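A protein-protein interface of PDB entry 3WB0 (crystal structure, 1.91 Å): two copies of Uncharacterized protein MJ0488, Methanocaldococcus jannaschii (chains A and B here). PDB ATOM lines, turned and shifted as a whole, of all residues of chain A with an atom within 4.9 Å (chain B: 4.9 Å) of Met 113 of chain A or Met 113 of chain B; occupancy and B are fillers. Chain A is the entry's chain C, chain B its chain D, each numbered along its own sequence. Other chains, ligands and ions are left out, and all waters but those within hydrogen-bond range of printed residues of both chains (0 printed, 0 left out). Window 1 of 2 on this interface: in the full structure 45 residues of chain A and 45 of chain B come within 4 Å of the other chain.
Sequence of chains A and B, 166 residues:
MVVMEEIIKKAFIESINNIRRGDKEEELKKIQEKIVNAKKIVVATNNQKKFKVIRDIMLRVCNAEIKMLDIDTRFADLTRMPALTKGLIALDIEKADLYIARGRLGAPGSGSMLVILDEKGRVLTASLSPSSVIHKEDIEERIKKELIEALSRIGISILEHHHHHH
N of Met 113 of chain A sits at hydrogen-bond distance from O of Gly 103 of chain A, 2.8 Å away.
O of Ser 127 of chain B is in hydrogen-bond range of N of Leu 114 of chain B.
The backbone carbonyl oxygen of Gly 111 of chain A sits at hydrogen-bond distance from the backbone NH of Leu 105 of chain A.
N of Leu 114 of chain A sits at hydrogen-bond distance from O of Ser 127 of chain A (2.8 Å).
The backbone carbonyl oxygen of Gly 103 of chain B lies within hydrogen-bond range of the backbone NH of Met 113 of chain B (2.7 Å).
The backbone NH of Leu 105 of chain B sits at hydrogen-bond distance from the backbone carbonyl oxygen of Gly 111 of chain B.
Among the printed residues, merely in contact across the chains: Leu 84 of chain A with Met 81 of chain B, Leu 105 of chain A with Ala 126 of chain B, Met 113 of chain A with Met 113 of chain B, Ala 126 of chain A with Leu 105 of chain B, Ala 126 of chain A with Leu 128 of chain B, Ser 127 of chain A with Leu 128 of chain B, Leu 128 of chain A with Ala 126 of chain B, Leu 128 of chain A with Ser 127 of chain B and Leu 128 of chain A with Leu 128 of chain B.
Of the printed residues of chain B, Leu 84 of chain A touches Met 81.
Of chain B, only Met 113 comes within 4 Å of Met 113 of chain A.
Val 115 of chain A touches none of the printed residues of chain B.
Of the printed residues of chain A, Met 81 of chain B touches Leu 84.
Gly 111 of chain B touches none of the printed residues of chain A.
Of the printed residues of chain A, Ala 126 of chain B touches Leu 105 and Leu 128.
Printed residues of chain A within 4 Å of Leu 128 of chain B: Ala 126, Ser 127 and Leu 128.
The nearest printed residue of chain A that does not touch Met 113 of chain B is Leu 105 of chain A (4.9 Å).
The nearest printed residue of chain B that does not touch Leu 128 of chain A is Met 113 of chain B (5.4 Å).
Of the 15 printed residues of chain B, 6 touch a printed residue of chain A.
Hydrophobic or aromatic side chains of chain A within 4 Å of the printed part of chain B: Leu 84, Leu 105, Met 113, Ala 126 and Leu 128.
Among the printed residues, no Asp or Glu carboxylate lies within 4 Å of a Lys or Arg side-chain nitrogen of the other chain.
Leu 105 of chain A touches Ala 126 of chain B, and with the chains exchanged Ala 126 of chain A touches Leu 105 of chain B.
Ala 126 of chain A touches Leu 128 of chain B, and with the chains exchanged Leu 128 of chain A touches Ala 126 of chain B.
Ser 127 of chain A touches Leu 128 of chain B, and with the chains exchanged Leu 128 of chain A touches Ser 127 of chain B.
Leu 128 of chain B touches its own counterpart, Leu 128 of chain A.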
ATOM      1  N   MET A  81      18.496  18.020  34.878  1.00  0.00           N
ATOM      2  CA  MET A  81      17.638  19.188  34.853  1.00  0.00           C
ATOM      3  C   MET A  81      16.858  19.168  36.136  1.00  0.00           C
ATOM      4  O   MET A  81      15.759  18.597  36.175  1.00  0.00           O
ATOM      5  CB  MET A  81      16.723  19.189  33.655  1.00  0.00           C
ATOM      6  CG  MET A  81      17.518  19.162  32.322  1.00  0.00           C
ATOM      7  SD  MET A  81      16.479  19.438  30.896  1.00  0.00           S
ATOM      8  CE  MET A  81      15.893  21.133  31.102  1.00  0.00           C
ATOM      9  N   ALA A  83      15.132  21.426  38.042  1.00  0.00           N
ATOM     10  CA  ALA A  83      13.776  21.973  38.113  1.00  0.00           C
ATOM     11  C   ALA A  83      12.747  20.978  37.586  1.00  0.00           C
ATOM     12  O   ALA A  83      11.695  20.750  38.203  1.00  0.00           O
ATOM     13  CB  ALA A  83      13.695  23.334  37.373  1.00  0.00           C
ATOM     14  N   LEU A  84      13.043  20.322  36.466  1.00  0.00           N
ATOM     15  CA  LEU A  84      12.113  19.318  35.889  1.00  0.00           C
ATOM     16  C   LEU A  84      11.979  18.122  36.824  1.00  0.00           C
ATOM     17  O   LEU A  84      10.864  17.699  37.090  1.00  0.00           O
ATOM     18  CB  LEU A  84      12.562  18.796  34.507  1.00  0.00           C
ATOM     19  CG  LEU A  84      11.483  18.580  33.393  1.00  0.00           C
ATOM     20  CD1 LEU A  84      10.093  17.991  33.720  1.00  0.00           C
ATOM     21  CD2 LEU A  84      11.216  19.912  32.685  1.00  0.00           C
ATOM     22  N   ALA A 101       7.372  23.932  39.714  1.00  0.00           N
ATOM     23  CA  ALA A 101       8.652  23.703  40.350  1.00  0.00           C
ATOM     24  C   ALA A 101       9.605  24.773  39.967  1.00  0.00           C
ATOM     25  O   ALA A 101       9.552  25.213  38.876  1.00  0.00           O
ATOM     26  CB  ALA A 101       9.227  22.344  39.940  1.00  0.00           C
ATOM     27  N   ARG A 102      10.525  25.157  40.864  1.00  0.00           N
ATOM     28  CA  ARG A 102      11.600  26.126  40.546  1.00  0.00           C
ATOM     29  C   ARG A 102      12.962  25.629  41.091  1.00  0.00           C
ATOM     30  O   ARG A 102      13.060  25.300  42.288  1.00  0.00           O
ATOM     31  CB  ARG A 102      11.315  27.491  41.170  1.00  0.00           C
ATOM     32  CG  ARG A 102      12.120  28.626  40.640  1.00  0.00           C
ATOM     33  CD  ARG A 102      13.262  29.074  41.477  1.00  0.00           C
ATOM     34  NE  ARG A 102      13.895  30.292  40.900  1.00  0.00           N
ATOM     35  CZ  ARG A 102      15.061  30.790  41.316  1.00  0.00           C
ATOM     36  NH1 ARG A 102      15.584  31.881  40.754  1.00  0.00           N
ATOM     37  NH2 ARG A 102      15.707  30.198  42.318  1.00  0.00           N
ATOM     38  N   GLY A 103      13.992  25.580  40.233  1.00  0.00           N
ATOM     39  CA  GLY A 103      15.294  25.048  40.637  1.00  0.00           C
ATOM     40  C   GLY A 103      16.315  25.404  39.593  1.00  0.00           C
ATOM     41  O   GLY A 103      16.047  26.253  38.734  1.00  0.00           O
ATOM     42  N   ARG A 104      17.537  24.875  39.732  1.00  0.00           N
ATOM     43  CA  ARG A 104      18.514  25.021  38.695  1.00  0.00           C
ATOM     44  C   ARG A 104      18.018  24.396  37.379  1.00  0.00           C
ATOM     45  O   ARG A 104      17.393  23.272  37.368  1.00  0.00           O
ATOM     46  CB  ARG A 104      19.873  24.451  39.164  1.00  0.00           C
ATOM     47  CG  ARG A 104      21.061  24.659  38.220  1.00  0.00           C
ATOM     48  CD  ARG A 104      22.392  24.203  38.838  1.00  0.00           C
ATOM     49  NE  ARG A 104      22.459  22.757  38.850  1.00  0.00           N
ATOM     50  CZ  ARG A 104      22.776  21.995  39.920  1.00  0.00           C
ATOM     51  NH1 ARG A 104      23.019  22.520  41.138  1.00  0.00           N
ATOM     52  NH2 ARG A 104      22.817  20.684  39.763  1.00  0.00           N
ATOM     53  N   LEU A 105      18.306  25.123  36.283  1.00  0.00           N
ATOM     54  CA  LEU A 105      18.000  24.717  34.909  1.00  0.00           C
ATOM     55  C   LEU A 105      18.742  23.413  34.579  1.00  0.00           C
ATOM     56  O   LEU A 105      18.155  22.422  34.149  1.00  0.00           O
ATOM     57  CB  LEU A 105      18.509  25.824  33.937  1.00  0.00           C
ATOM     58  CG  LEU A 105      18.573  25.556  32.391  1.00  0.00           C
ATOM     59  CD1 LEU A 105      17.216  25.092  31.836  1.00  0.00           C
ATOM     60  CD2 LEU A 105      19.133  26.720  31.495  1.00  0.00           C
ATOM     61  N   GLY A 111      21.980  28.757  35.946  1.00  0.00           N
ATOM     62  CA  GLY A 111      20.888  29.656  36.325  1.00  0.00           C
ATOM     63  C   GLY A 111      19.635  28.873  36.656  1.00  0.00           C
ATOM     64  O   GLY A 111      19.667  27.570  36.812  1.00  0.00           O
ATOM     65  N   SER A 112      18.517  29.629  36.733  1.00  0.00           N
ATOM     66  CA  SER A 112      17.284  29.029  37.253  1.00  0.00           C
ATOM     67  C   SER A 112      16.205  28.752  36.179  1.00  0.00           C
ATOM     68  O   SER A 112      16.200  29.396  35.133  1.00  0.00           O
ATOM     69  CB  SER A 112      16.711  29.913  38.335  1.00  0.00           C
ATOM     70  OG  SER A 112      16.092  30.983  37.651  1.00  0.00           O
ATOM     71  N   MET A 113      15.339  27.772  36.460  1.00  0.00           N
ATOM     72  CA  MET A 113      14.131  27.448  35.680  1.00  0.00           C
ATOM     73  C   MET A 113      12.920  27.315  36.611  1.00  0.00           C
ATOM     74  O   MET A 113      13.010  26.629  37.625  1.00  0.00           O
ATOM     75  CB  MET A 113      14.299  26.135  34.895  1.00  0.00           C
ATOM     76  CG  MET A 113      13.034  25.703  34.180  1.00  0.00           C
ATOM     77  SD  MET A 113      13.083  24.110  33.356  1.00  0.00           S
ATOM     78  CE  MET A 113      13.528  24.609  31.715  1.00  0.00           C
ATOM     79  N   LEU A 114      11.797  27.962  36.283  1.00  0.00           N
ATOM     80  CA  LEU A 114      10.491  27.686  36.931  1.00  0.00           C
ATOM     81  C   LEU A 114       9.658  26.939  35.830  1.00  0.00           C
ATOM     82  O   LEU A 114       9.669  27.365  34.684  1.00  0.00           O
ATOM     83  CB  LEU A 114       9.792  28.968  37.318  1.00  0.00           C
ATOM     84  CG  LEU A 114       8.351  28.875  37.920  1.00  0.00           C
ATOM     85  CD1 LEU A 114       8.088  30.025  38.868  1.00  0.00           C
ATOM     86  CD2 LEU A 114       7.213  28.751  36.916  1.00  0.00           C
ATOM     87  N   VAL A 115       9.032  25.825  36.171  1.00  0.00           N
ATOM     88  CA  VAL A 115       8.282  25.056  35.189  1.00  0.00           C
ATOM     89  C   VAL A 115       6.898  24.748  35.726  1.00  0.00           C
ATOM     90  O   VAL A 115       6.769  24.538  36.865  1.00  0.00           O
ATOM     91  CB  VAL A 115       9.049  23.771  34.820  1.00  0.00           C
ATOM     92  CG1 VAL A 115       9.431  22.967  36.072  1.00  0.00           C
ATOM     93  CG2 VAL A 115       8.308  22.945  33.758  1.00  0.00           C
ATOM     94  N   ALA A 126       7.365  27.584  31.162  1.00  0.00           N
ATOM     95  CA  ALA A 126       8.557  27.675  32.038  1.00  0.00           C
ATOM     96  C   ALA A 126       9.096  29.063  31.863  1.00  0.00           C
ATOM     97  O   ALA A 126       8.733  29.738  30.879  1.00  0.00           O
ATOM     98  CB  ALA A 126       9.653  26.690  31.573  1.00  0.00           C
ATOM     99  N   SER A 127       9.949  29.520  32.797  1.00  0.00           N
ATOM    100  CA  SER A 127      10.775  30.649  32.513  1.00  0.00           C
ATOM    101  C   SER A 127      12.093  30.494  33.249  1.00  0.00           C
ATOM    102  O   SER A 127      12.205  29.680  34.166  1.00  0.00           O
ATOM    103  CB  SER A 127      10.111  31.963  32.889  1.00  0.00           C
ATOM    104  OG  SER A 127       9.877  31.954  34.247  1.00  0.00           O
ATOM    105  N   LEU A 128      13.078  31.273  32.808  1.00  0.00           N
ATOM    106  CA  LEU A 128      14.464  31.143  33.251  1.00  0.00           C
ATOM    107  C   LEU A 128      14.893  32.505  33.802  1.00  0.00           C
ATOM    108  O   LEU A 128      14.421  33.569  33.302  1.00  0.00           O
ATOM    109  CB  LEU A 128      15.379  30.810  32.055  1.00  0.00           C
ATOM    110  CG  LEU A 128      14.874  29.657  31.172  1.00  0.00           C
ATOM    111  CD1 LEU A 128      15.848  29.476  30.032  1.00  0.00           C
ATOM    112  CD2 LEU A 128      14.691  28.340  31.959  1.00  0.00           C
ATOM    113  N   MET B  81       9.848  17.110  25.360  1.00  0.00           N
ATOM    114  CA  MET B  81      10.603  18.321  25.314  1.00  0.00           C
ATOM    115  C   MET B  81      11.408  18.263  24.030  1.00  0.00           C
ATOM    116  O   MET B  81      12.534  17.849  23.998  1.00  0.00           O
ATOM    117  CB  MET B  81      11.499  18.465  26.536  1.00  0.00           C
ATOM    118  CG  MET B  81      10.692  18.801  27.785  1.00  0.00           C
ATOM    119  SD  MET B  81      11.757  19.158  29.183  1.00  0.00           S
ATOM    120  CE  MET B  81      12.021  20.903  28.906  1.00  0.00           C
ATOM    121  N   ALA B  83      12.966  20.456  21.809  1.00  0.00           N
ATOM    122  CA  ALA B  83      14.285  21.119  21.661  1.00  0.00           C
ATOM    123  C   ALA B  83      15.352  20.275  22.279  1.00  0.00           C
ATOM    124  O   ALA B  83      16.387  20.051  21.676  1.00  0.00           O
ATOM    125  CB  ALA B  83      14.316  22.470  22.362  1.00  0.00           C
ATOM    126  N   ALA B 101      20.450  23.576  19.872  1.00  0.00           N
ATOM    127  CA  ALA B 101      19.179  23.179  19.324  1.00  0.00           C
ATOM    128  C   ALA B 101      18.112  24.185  19.591  1.00  0.00           C
ATOM    129  O   ALA B 101      18.069  24.839  20.643  1.00  0.00           O
ATOM    130  CB  ALA B 101      18.755  21.803  19.847  1.00  0.00           C
ATOM    131  N   ARG B 102      17.226  24.325  18.634  1.00  0.00           N
ATOM    132  CA  ARG B 102      16.090  25.161  18.868  1.00  0.00           C
ATOM    133  C   ARG B 102      14.833  24.473  18.392  1.00  0.00           C
ATOM    134  O   ARG B 102      14.748  23.965  17.253  1.00  0.00           O
ATOM    135  CB  ARG B 102      16.274  26.520  18.215  1.00  0.00           C
ATOM    136  CG  ARG B 102      15.292  27.575  18.745  1.00  0.00           C
ATOM    137  CD  ARG B 102      14.218  27.943  17.744  1.00  0.00           C
ATOM    138  NE  ARG B 102      13.465  29.154  18.087  1.00  0.00           N
ATOM    139  CZ  ARG B 102      12.258  29.477  17.600  1.00  0.00           C
ATOM    140  NH1 ARG B 102      11.642  30.623  17.952  1.00  0.00           N
ATOM    141  NH2 ARG B 102      11.621  28.652  16.783  1.00  0.00           N
ATOM    142  N   GLY B 103      13.860  24.416  19.269  1.00  0.00           N
ATOM    143  CA  GLY B 103      12.495  23.937  18.860  1.00  0.00           C
ATOM    144  C   GLY B 103      11.447  24.194  19.931  1.00  0.00           C
ATOM    145  O   GLY B 103      11.609  25.105  20.755  1.00  0.00           O
ATOM    146  N   ARG B 104      10.345  23.436  19.917  1.00  0.00           N
ATOM    147  CA  ARG B 104       9.307  23.635  20.927  1.00  0.00           C
ATOM    148  C   ARG B 104       9.790  23.222  22.354  1.00  0.00           C
ATOM    149  O   ARG B 104      10.456  22.195  22.510  1.00  0.00           O
ATOM    150  CB  ARG B 104       8.110  22.779  20.575  1.00  0.00           C
ATOM    151  CG  ARG B 104       6.900  23.015  21.461  1.00  0.00           C
ATOM    152  CD  ARG B 104       5.724  22.433  20.766  1.00  0.00           C
ATOM    153  NE  ARG B 104       5.666  21.005  21.003  1.00  0.00           N
ATOM    154  CZ  ARG B 104       5.347  20.123  20.052  1.00  0.00           C
ATOM    155  NH1 ARG B 104       5.198  20.517  18.768  1.00  0.00           N
ATOM    156  NH2 ARG B 104       5.327  18.848  20.374  1.00  0.00           N
ATOM    157  N   LEU B 105       9.377  23.990  23.370  1.00  0.00           N
ATOM    158  CA  LEU B 105       9.742  23.736  24.766  1.00  0.00           C
ATOM    159  C   LEU B 105       9.207  22.400  25.270  1.00  0.00           C
ATOM    160  O   LEU B 105       9.962  21.574  25.746  1.00  0.00           O
ATOM    161  CB  LEU B 105       9.191  24.895  25.633  1.00  0.00           C
ATOM    162  CG  LEU B 105       9.190  24.632  27.118  1.00  0.00           C
ATOM    163  CD1 LEU B 105      10.654  24.573  27.691  1.00  0.00           C
ATOM    164  CD2 LEU B 105       8.325  25.614  27.882  1.00  0.00           C
ATOM    165  N   GLY B 111       5.376  27.264  23.224  1.00  0.00           N
ATOM    166  CA  GLY B 111       6.447  28.227  22.800  1.00  0.00           C
ATOM    167  C   GLY B 111       7.766  27.514  22.568  1.00  0.00           C
ATOM    168  O   GLY B 111       7.788  26.263  22.454  1.00  0.00           O
ATOM    169  N   SER B 112       8.863  28.253  22.526  1.00  0.00           N
ATOM    170  CA  SER B 112      10.087  27.733  21.964  1.00  0.00           C
ATOM    171  C   SER B 112      11.186  27.742  23.004  1.00  0.00           C
ATOM    172  O   SER B 112      11.142  28.534  23.952  1.00  0.00           O
ATOM    173  CB  SER B 112      10.522  28.672  20.834  1.00  0.00           C
ATOM    174  OG  SER B 112      10.918  29.924  21.389  1.00  0.00           O
ATOM    175  N   MET B 113      12.170  26.860  22.792  1.00  0.00           N
ATOM    176  CA  MET B 113      13.347  26.750  23.648  1.00  0.00           C
ATOM    177  C   MET B 113      14.586  26.635  22.784  1.00  0.00           C
ATOM    178  O   MET B 113      14.595  25.856  21.844  1.00  0.00           O
ATOM    179  CB  MET B 113      13.299  25.443  24.501  1.00  0.00           C
ATOM    180  CG  MET B 113      14.646  25.255  25.284  1.00  0.00           C
ATOM    181  SD  MET B 113      14.559  23.882  26.438  1.00  0.00           S
ATOM    182  CE  MET B 113      14.218  24.819  27.908  1.00  0.00           C
ATOM    183  N   LEU B 114      15.651  27.327  23.128  1.00  0.00           N
ATOM    184  CA  LEU B 114      16.903  27.110  22.418  1.00  0.00           C
ATOM    185  C   LEU B 114      17.785  26.684  23.508  1.00  0.00           C
ATOM    186  O   LEU B 114      17.748  27.270  24.567  1.00  0.00           O
ATOM    187  CB  LEU B 114      17.392  28.452  21.794  1.00  0.00           C
ATOM    188  CG  LEU B 114      18.786  28.510  21.212  1.00  0.00           C
ATOM    189  CD1 LEU B 114      18.961  29.600  20.149  1.00  0.00           C
ATOM    190  CD2 LEU B 114      19.792  28.819  22.306  1.00  0.00           C
ATOM    191  N   VAL B 115      18.577  25.634  23.273  1.00  0.00           N
ATOM    192  CA  VAL B 115      19.393  25.044  24.341  1.00  0.00           C
ATOM    193  C   VAL B 115      20.775  24.776  23.799  1.00  0.00           C
ATOM    194  O   VAL B 115      20.936  24.510  22.608  1.00  0.00           O
ATOM    195  CB  VAL B 115      18.684  23.809  24.950  1.00  0.00           C
ATOM    196  CG1 VAL B 115      18.489  22.730  23.883  1.00  0.00           C
ATOM    197  CG2 VAL B 115      19.407  23.318  26.178  1.00  0.00           C
ATOM    198  N   ALA B 126      20.034  28.000  28.156  1.00  0.00           N
ATOM    199  CA  ALA B 126      18.837  27.914  27.315  1.00  0.00           C
ATOM    200  C   ALA B 126      18.170  29.274  27.327  1.00  0.00           C
ATOM    201  O   ALA B 126      18.518  30.115  28.136  1.00  0.00           O
ATOM    202  CB  ALA B 126      17.890  26.829  27.857  1.00  0.00           C
ATOM    203  N   SER B 127      17.218  29.500  26.443  1.00  0.00           N
ATOM    204  CA  SER B 127      16.364  30.665  26.544  1.00  0.00           C
ATOM    205  C   SER B 127      15.087  30.320  25.803  1.00  0.00           C
ATOM    206  O   SER B 127      15.051  29.362  25.025  1.00  0.00           O
ATOM    207  CB  SER B 127      16.967  31.950  25.963  1.00  0.00           C
ATOM    208  OG  SER B 127      17.157  31.771  24.604  1.00  0.00           O
ATOM    209  N   LEU B 128      14.032  31.071  26.104  1.00  0.00           N
ATOM    210  CA  LEU B 128      12.697  30.692  25.673  1.00  0.00           C
ATOM    211  C   LEU B 128      12.096  31.881  24.927  1.00  0.00           C
ATOM    212  O   LEU B 128      12.485  33.033  25.238  1.00  0.00           O
ATOM    213  CB  LEU B 128      11.853  30.354  26.907  1.00  0.00           C
ATOM    214  CG  LEU B 128      12.403  29.319  27.897  1.00  0.00           C
ATOM    215  CD1 LEU B 128      11.586  29.186  29.211  1.00  0.00           C
ATOM    216  CD2 LEU B 128      12.487  27.974  27.210  1.00  0.00           C
